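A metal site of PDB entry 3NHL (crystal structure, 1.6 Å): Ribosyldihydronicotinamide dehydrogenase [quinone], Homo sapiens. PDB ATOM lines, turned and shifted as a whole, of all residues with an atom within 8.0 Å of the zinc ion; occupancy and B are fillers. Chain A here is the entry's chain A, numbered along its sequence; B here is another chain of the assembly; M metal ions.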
ATOM      1  N   TYR A 132      26.898  25.270 -20.560  1.00  0.00           N
ATOM      2  CA  TYR A 132      26.256  24.350 -19.651  1.00  0.00           C
ATOM      3  C   TYR A 132      26.821  22.923 -19.873  1.00  0.00           C
ATOM      4  O   TYR A 132      28.055  22.755 -19.843  1.00  0.00           O
ATOM      5  CB  TYR A 132      24.716  24.464 -19.700  1.00  0.00           C
ATOM      6  CG  TYR A 132      24.298  25.750 -18.947  1.00  0.00           C
ATOM      7  CD1 TYR A 132      24.722  25.954 -17.633  1.00  0.00           C
ATOM      8  CD2 TYR A 132      23.537  26.751 -19.561  1.00  0.00           C
ATOM      9  CE1 TYR A 132      24.382  27.146 -16.935  1.00  0.00           C
ATOM     10  CE2 TYR A 132      23.151  27.940 -18.863  1.00  0.00           C
ATOM     11  CZ  TYR A 132      23.607  28.092 -17.558  1.00  0.00           C
ATOM     12  OH  TYR A 132      23.268  29.284 -16.911  1.00  0.00           O
ATOM     13  N   ASP A 133      25.971  21.909 -20.045  1.00  0.00           N
ATOM     14  CA  ASP A 133      26.435  20.562 -20.363  1.00  0.00           C
ATOM     15  C   ASP A 133      27.494  20.420 -21.478  1.00  0.00           C
ATOM     16  O   ASP A 133      28.341  19.470 -21.457  1.00  0.00           O
ATOM     17  CB  ASP A 133      25.219  19.688 -20.681  1.00  0.00           C
ATOM     18  CG  ASP A 133      24.474  19.285 -19.443  1.00  0.00           C
ATOM     19  OD1 ASP A 133      24.842  19.797 -18.377  1.00  0.00           O
ATOM     20  OD2 ASP A 133      23.529  18.448 -19.494  1.00  0.00           O
ATOM     21  N   TRP A 169      24.492  29.115  -6.320  1.00  0.00           N
ATOM     22  CA  TRP A 169      24.014  29.189  -7.657  1.00  0.00           C
ATOM     23  C   TRP A 169      24.882  29.946  -8.679  1.00  0.00           C
ATOM     24  O   TRP A 169      25.147  29.416  -9.756  1.00  0.00           O
ATOM     25  CB  TRP A 169      22.505  29.709  -7.647  1.00  0.00           C
ATOM     26  CG  TRP A 169      21.841  29.943  -8.967  1.00  0.00           C
ATOM     27  CD1 TRP A 169      21.558  31.183  -9.537  1.00  0.00           C
ATOM     28  CD2 TRP A 169      21.277  28.973  -9.855  1.00  0.00           C
ATOM     29  NE1 TRP A 169      20.885  31.015 -10.745  1.00  0.00           N
ATOM     30  CE2 TRP A 169      20.704  29.659 -10.955  1.00  0.00           C
ATOM     31  CE3 TRP A 169      21.229  27.556  -9.827  1.00  0.00           C
ATOM     32  CZ2 TRP A 169      20.039  28.985 -12.029  1.00  0.00           C
ATOM     33  CZ3 TRP A 169      20.619  26.889 -10.899  1.00  0.00           C
ATOM     34  CH2 TRP A 169      19.991  27.614 -11.965  1.00  0.00           C
ATOM     35  N   LEU A 171      27.901  30.630  -8.612  1.00  0.00           N
ATOM     36  CA  LEU A 171      29.251  29.988  -8.740  1.00  0.00           C
ATOM     37  C   LEU A 171      29.161  28.574  -9.347  1.00  0.00           C
ATOM     38  O   LEU A 171      29.784  28.388 -10.364  1.00  0.00           O
ATOM     39  CB  LEU A 171      29.888  29.922  -7.358  1.00  0.00           C
ATOM     40  CG  LEU A 171      30.207  31.269  -6.637  1.00  0.00           C
ATOM     41  CD1 LEU A 171      30.696  31.053  -5.270  1.00  0.00           C
ATOM     42  CD2 LEU A 171      31.212  32.092  -7.478  1.00  0.00           C
ATOM     43  N   GLN A 172      28.317  27.732  -8.761  1.00  0.00           N
ATOM     44  CA  GLN A 172      28.214  26.369  -9.293  1.00  0.00           C
ATOM     45  C   GLN A 172      27.562  26.348 -10.616  1.00  0.00           C
ATOM     46  O   GLN A 172      28.065  25.767 -11.597  1.00  0.00           O
ATOM     47  CB  GLN A 172      27.545  25.492  -8.324  1.00  0.00           C
ATOM     48  CG  GLN A 172      28.365  25.226  -7.170  1.00  0.00           C
ATOM     49  CD  GLN A 172      27.783  24.190  -6.291  1.00  0.00           C
ATOM     50  OE1 GLN A 172      26.510  23.961  -6.277  1.00  0.00           O
ATOM     51  NE2 GLN A 172      28.635  23.642  -5.416  1.00  0.00           N
ATOM     52  N   HIS A 173      26.391  27.006 -10.705  1.00  0.00           N
ATOM     53  CA  HIS A 173      25.640  27.000 -11.955  1.00  0.00           C
ATOM     54  C   HIS A 173      26.054  28.011 -12.944  1.00  0.00           C
ATOM     55  O   HIS A 173      26.434  27.748 -14.073  1.00  0.00           O
ATOM     56  CB  HIS A 173      24.097  27.094 -11.689  1.00  0.00           C
ATOM     57  CG  HIS A 173      23.272  26.922 -12.930  1.00  0.00           C
ATOM     58  ND1 HIS A 173      23.038  25.692 -13.508  1.00  0.00           N
ATOM     59  CD2 HIS A 173      22.635  27.828 -13.723  1.00  0.00           C
ATOM     60  CE1 HIS A 173      22.324  25.845 -14.610  1.00  0.00           C
ATOM     61  NE2 HIS A 173      22.046  27.128 -14.763  1.00  0.00           N
ATOM     62  N   GLY A 174      25.993  29.271 -12.550  1.00  0.00           N
ATOM     63  CA  GLY A 174      26.293  30.300 -13.500  1.00  0.00           C
ATOM     64  C   GLY A 174      27.730  30.385 -13.956  1.00  0.00           C
ATOM     65  O   GLY A 174      27.952  30.972 -14.978  1.00  0.00           O
ATOM     66  N   THR A 175      28.655  29.796 -13.183  1.00  0.00           N
ATOM     67  CA  THR A 175      30.061  29.887 -13.624  1.00  0.00           C
ATOM     68  C   THR A 175      30.557  28.467 -13.952  1.00  0.00           C
ATOM     69  O   THR A 175      30.875  28.249 -15.120  1.00  0.00           O
ATOM     70  CB  THR A 175      30.943  30.498 -12.530  1.00  0.00           C
ATOM     71  OG1 THR A 175      30.345  31.783 -12.196  1.00  0.00           O
ATOM     72  CG2 THR A 175      32.356  30.740 -13.088  1.00  0.00           C
ATOM     73  N   LEU A 176      30.553  27.554 -13.030  1.00  0.00           N
ATOM     74  CA  LEU A 176      31.300  26.226 -13.306  1.00  0.00           C
ATOM     75  C   LEU A 176      30.529  25.334 -14.323  1.00  0.00           C
ATOM     76  O   LEU A 176      31.045  25.044 -15.383  1.00  0.00           O
ATOM     77  CB  LEU A 176      31.568  25.511 -12.059  1.00  0.00           C
ATOM     78  CG  LEU A 176      32.447  26.303 -11.019  1.00  0.00           C
ATOM     79  CD1 LEU A 176      32.584  25.551  -9.773  1.00  0.00           C
ATOM     80  CD2 LEU A 176      33.779  26.647 -11.655  1.00  0.00           C
ATOM     81  N   HIS A 177      29.228  25.162 -14.063  1.00  0.00           N
ATOM     82  CA  HIS A 177      28.373  24.419 -15.031  1.00  0.00           C
ATOM     83  C   HIS A 177      28.368  25.059 -16.363  1.00  0.00           C
ATOM     84  O   HIS A 177      28.458  24.422 -17.437  1.00  0.00           O
ATOM     85  CB  HIS A 177      26.973  24.276 -14.419  1.00  0.00           C
ATOM     86  CG  HIS A 177      26.075  23.319 -15.181  1.00  0.00           C
ATOM     87  ND1 HIS A 177      24.828  22.985 -14.701  1.00  0.00           N
ATOM     88  CD2 HIS A 177      26.255  22.616 -16.325  1.00  0.00           C
ATOM     89  CE1 HIS A 177      24.235  22.159 -15.560  1.00  0.00           C
ATOM     90  NE2 HIS A 177      25.086  21.882 -16.537  1.00  0.00           N
ATOM     91  N   PHE A 178      28.208  26.373 -16.406  1.00  0.00           N
ATOM     92  CA  PHE A 178      28.171  27.056 -17.576  1.00  0.00           C
ATOM     93  C   PHE A 178      29.365  26.740 -18.444  1.00  0.00           C
ATOM     94  O   PHE A 178      29.245  26.681 -19.616  1.00  0.00           O
ATOM     95  CB  PHE A 178      27.959  28.618 -17.327  1.00  0.00           C
ATOM     96  CG  PHE A 178      27.824  29.406 -18.610  1.00  0.00           C
ATOM     97  CD1 PHE A 178      26.497  29.675 -19.153  1.00  0.00           C
ATOM     98  CD2 PHE A 178      28.892  29.867 -19.291  1.00  0.00           C
ATOM     99  CE1 PHE A 178      26.368  30.409 -20.389  1.00  0.00           C
ATOM    100  CE2 PHE A 178      28.835  30.562 -20.413  1.00  0.00           C
ATOM    101  CZ  PHE A 178      27.519  30.847 -21.075  1.00  0.00           C
ATOM    102  N   PHE A 181      32.126  22.268 -16.549  1.00  0.00           N
ATOM    103  CA  PHE A 181      32.466  21.420 -15.424  1.00  0.00           C
ATOM    104  C   PHE A 181      31.337  20.581 -14.918  1.00  0.00           C
ATOM    105  O   PHE A 181      30.198  21.043 -14.815  1.00  0.00           O
ATOM    106  CB  PHE A 181      32.958  22.242 -14.186  1.00  0.00           C
ATOM    107  CG  PHE A 181      34.272  22.992 -14.414  1.00  0.00           C
ATOM    108  CD1 PHE A 181      35.494  22.329 -14.284  1.00  0.00           C
ATOM    109  CD2 PHE A 181      34.297  24.370 -14.668  1.00  0.00           C
ATOM    110  CE1 PHE A 181      36.721  22.986 -14.479  1.00  0.00           C
ATOM    111  CE2 PHE A 181      35.546  25.063 -14.844  1.00  0.00           C
ATOM    112  CZ  PHE A 181      36.767  24.285 -14.736  1.00  0.00           C
ATOM    113  N   VAL A 183      30.274  19.499 -11.465  1.00  0.00           N
ATOM    114  CA  VAL A 183      30.460  20.006 -10.150  1.00  0.00           C
ATOM    115  C   VAL A 183      30.309  19.003  -9.063  1.00  0.00           C
ATOM    116  O   VAL A 183      29.194  18.431  -8.763  1.00  0.00           O
ATOM    117  CB  VAL A 183      29.481  21.217  -9.905  1.00  0.00           C
ATOM    118  CG1 VAL A 183      29.758  21.888  -8.605  1.00  0.00           C
ATOM    119  CG2 VAL A 183      29.543  22.147 -11.121  1.00  0.00           C
ATOM    120  N   ILE A 220      27.185  16.385  -8.796  1.00  0.00           N
ATOM    121  CA  ILE A 220      25.800  16.817  -8.543  1.00  0.00           C
ATOM    122  C   ILE A 220      25.020  17.102  -9.841  1.00  0.00           C
ATOM    123  O   ILE A 220      25.592  17.332 -10.908  1.00  0.00           O
ATOM    124  CB  ILE A 220      25.731  18.011  -7.592  1.00  0.00           C
ATOM    125  CG1 ILE A 220      26.185  19.299  -8.297  1.00  0.00           C
ATOM    126  CG2 ILE A 220      26.544  17.720  -6.359  1.00  0.00           C
ATOM    127  CD1 ILE A 220      25.810  20.630  -7.623  1.00  0.00           C
ATOM    128  N   PRO A 221      23.670  17.025  -9.766  1.00  0.00           N
ATOM    129  CA  PRO A 221      22.872  17.497 -10.905  1.00  0.00           C
ATOM    130  C   PRO A 221      22.826  19.013 -10.697  1.00  0.00           C
ATOM    131  O   PRO A 221      22.260  19.458  -9.682  1.00  0.00           O
ATOM    132  CB  PRO A 221      21.485  16.855 -10.671  1.00  0.00           C
ATOM    133  CG  PRO A 221      21.393  16.654  -9.180  1.00  0.00           C
ATOM    134  CD  PRO A 221      22.857  16.355  -8.734  1.00  0.00           C
ATOM    135  N   CYS A 222      23.465  19.761 -11.593  1.00  0.00           N
ATOM    136  CA  CYS A 222      23.619  21.206 -11.329  1.00  0.00           C
ATOM    137  C   CYS A 222      22.408  21.938 -11.902  1.00  0.00           C
ATOM    138  O   CYS A 222      22.449  22.481 -13.030  1.00  0.00           O
ATOM    139  CB  CYS A 222      24.974  21.701 -11.842  1.00  0.00           C
ATOM    140  SG  CYS A 222      25.257  23.468 -11.497  1.00  0.00           S
ATOM    141  N   THR A 223      21.331  21.860 -11.143  1.00  0.00           N
ATOM    142  CA  THR A 223      20.023  22.369 -11.595  1.00  0.00           C
ATOM    143  C   THR A 223      19.408  23.357 -10.638  1.00  0.00           C
ATOM    144  O   THR A 223      19.742  23.385  -9.454  1.00  0.00           O
ATOM    145  CB  THR A 223      18.992  21.188 -11.752  1.00  0.00           C
ATOM    146  OG1 THR A 223      18.730  20.640 -10.446  1.00  0.00           O
ATOM    147  CG2 THR A 223      19.557  20.139 -12.664  1.00  0.00           C
ATOM    148  N   ALA A 224      18.456  24.140 -11.140  1.00  0.00           N
ATOM    149  CA  ALA A 224      17.700  25.060 -10.261  1.00  0.00           C
ATOM    150  C   ALA A 224      17.044  24.284  -9.114  1.00  0.00           C
ATOM    151  O   ALA A 224      17.090  24.690  -7.942  1.00  0.00           O
ATOM    152  CB  ALA A 224      16.652  25.856 -11.090  1.00  0.00           C
ATOM    153  N   TRP A 226      18.165  21.369  -7.799  1.00  0.00           N
ATOM    154  CA  TRP A 226      19.184  21.075  -6.759  1.00  0.00           C
ATOM    155  C   TRP A 226      19.453  22.272  -5.807  1.00  0.00           C
ATOM    156  O   TRP A 226      19.567  22.123  -4.576  1.00  0.00           O
ATOM    157  CB  TRP A 226      20.522  20.544  -7.371  1.00  0.00           C
ATOM    158  CG  TRP A 226      21.540  20.055  -6.321  1.00  0.00           C
ATOM    159  CD1 TRP A 226      21.692  18.788  -5.864  1.00  0.00           C
ATOM    160  CD2 TRP A 226      22.510  20.858  -5.600  1.00  0.00           C
ATOM    161  NE1 TRP A 226      22.671  18.733  -4.901  1.00  0.00           N
ATOM    162  CE2 TRP A 226      23.201  19.983  -4.721  1.00  0.00           C
ATOM    163  CE3 TRP A 226      22.842  22.214  -5.595  1.00  0.00           C
ATOM    164  CZ2 TRP A 226      24.221  20.415  -3.863  1.00  0.00           C
ATOM    165  CZ3 TRP A 226      23.850  22.663  -4.728  1.00  0.00           C
ATOM    166  CH2 TRP A 226      24.542  21.765  -3.892  1.00  0.00           C
ATOM    167  N   HIS A 227      19.542  23.464  -6.395  1.00  0.00           N
ATOM    168  CA  HIS A 227      19.821  24.653  -5.596  1.00  0.00           C
ATOM    169  C   HIS A 227      18.644  25.184  -4.754  1.00  0.00           C
ATOM    170  O   HIS A 227      18.838  25.613  -3.610  1.00  0.00           O
ATOM    171  CB  HIS A 227      20.397  25.754  -6.501  1.00  0.00           C
ATOM    172  CG  HIS A 227      21.760  25.421  -7.046  1.00  0.00           C
ATOM    173  ND1 HIS A 227      21.949  24.655  -8.184  1.00  0.00           N
ATOM    174  CD2 HIS A 227      22.997  25.774  -6.613  1.00  0.00           C
ATOM    175  CE1 HIS A 227      23.255  24.557  -8.430  1.00  0.00           C
ATOM    176  NE2 HIS A 227      23.911  25.213  -7.462  1.00  0.00           N
ATOM    177  N   VAL B 160      17.273  28.840 -19.611  1.00  0.00           N
ATOM    178  CA  VAL B 160      18.554  28.154 -19.347  1.00  0.00           C
ATOM    179  C   VAL B 160      19.217  28.602 -18.070  1.00  0.00           C
ATOM    180  O   VAL B 160      19.837  27.834 -17.278  1.00  0.00           O
ATOM    181  CB  VAL B 160      19.583  28.497 -20.429  1.00  0.00           C
ATOM    182  CG1 VAL B 160      19.941  27.280 -21.228  1.00  0.00           C
ATOM    183  CG2 VAL B 160      19.101  29.658 -21.275  1.00  0.00           C
HETATM  184 ZN    ZN M   1      24.012  23.938 -13.235  1.00  0.00          ZN
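ND1 of His 177 is bound to the zinc ion (1.9 Å). The zinc ion is bound by ND1 of His 173, at 2.0 Å. The zinc ion is bound by O of Cys 222, 2.1 Å away. The zinc ion is bound by SG of Cys 222, 2.2 Å away. The zinc ion has four donor atoms within binding distance.
Thr 223 touches the zinc ion. Of the 21 residues printed, 4 come within 4 Å of the zinc ion. The nearest printed residue that does not touch the zinc ion is Gln 172 (4.7 Å).
NE2 of His 173 lies within hydrogen-bond range of O of Val 160 of chain B, at 3.4 Å. O of His 173 sits at hydrogen-bond distance from N of Phe 178. A ring nitrogen (NE2) of His 173 sits close to the side-chain hydroxyl of Tyr 132 (3.3 Å). The side-chain sulfur (SG) of Cys 222 sits close to the backbone carbonyl oxygen (O) of Gln 172 (3.6 Å). OD1 of Asp 133 is in hydrogen-bond range of NE2 of His 177. OG1 of Thr 223 is in hydrogen-bond range of N of Trp 226 (2.8 Å). O of Thr 223 lies within hydrogen-bond range of ND1 of His 227. The backbone NH of His 177 is in hydrogen-bond range of the backbone carbonyl oxygen of Gln 172 (2.8 Å).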
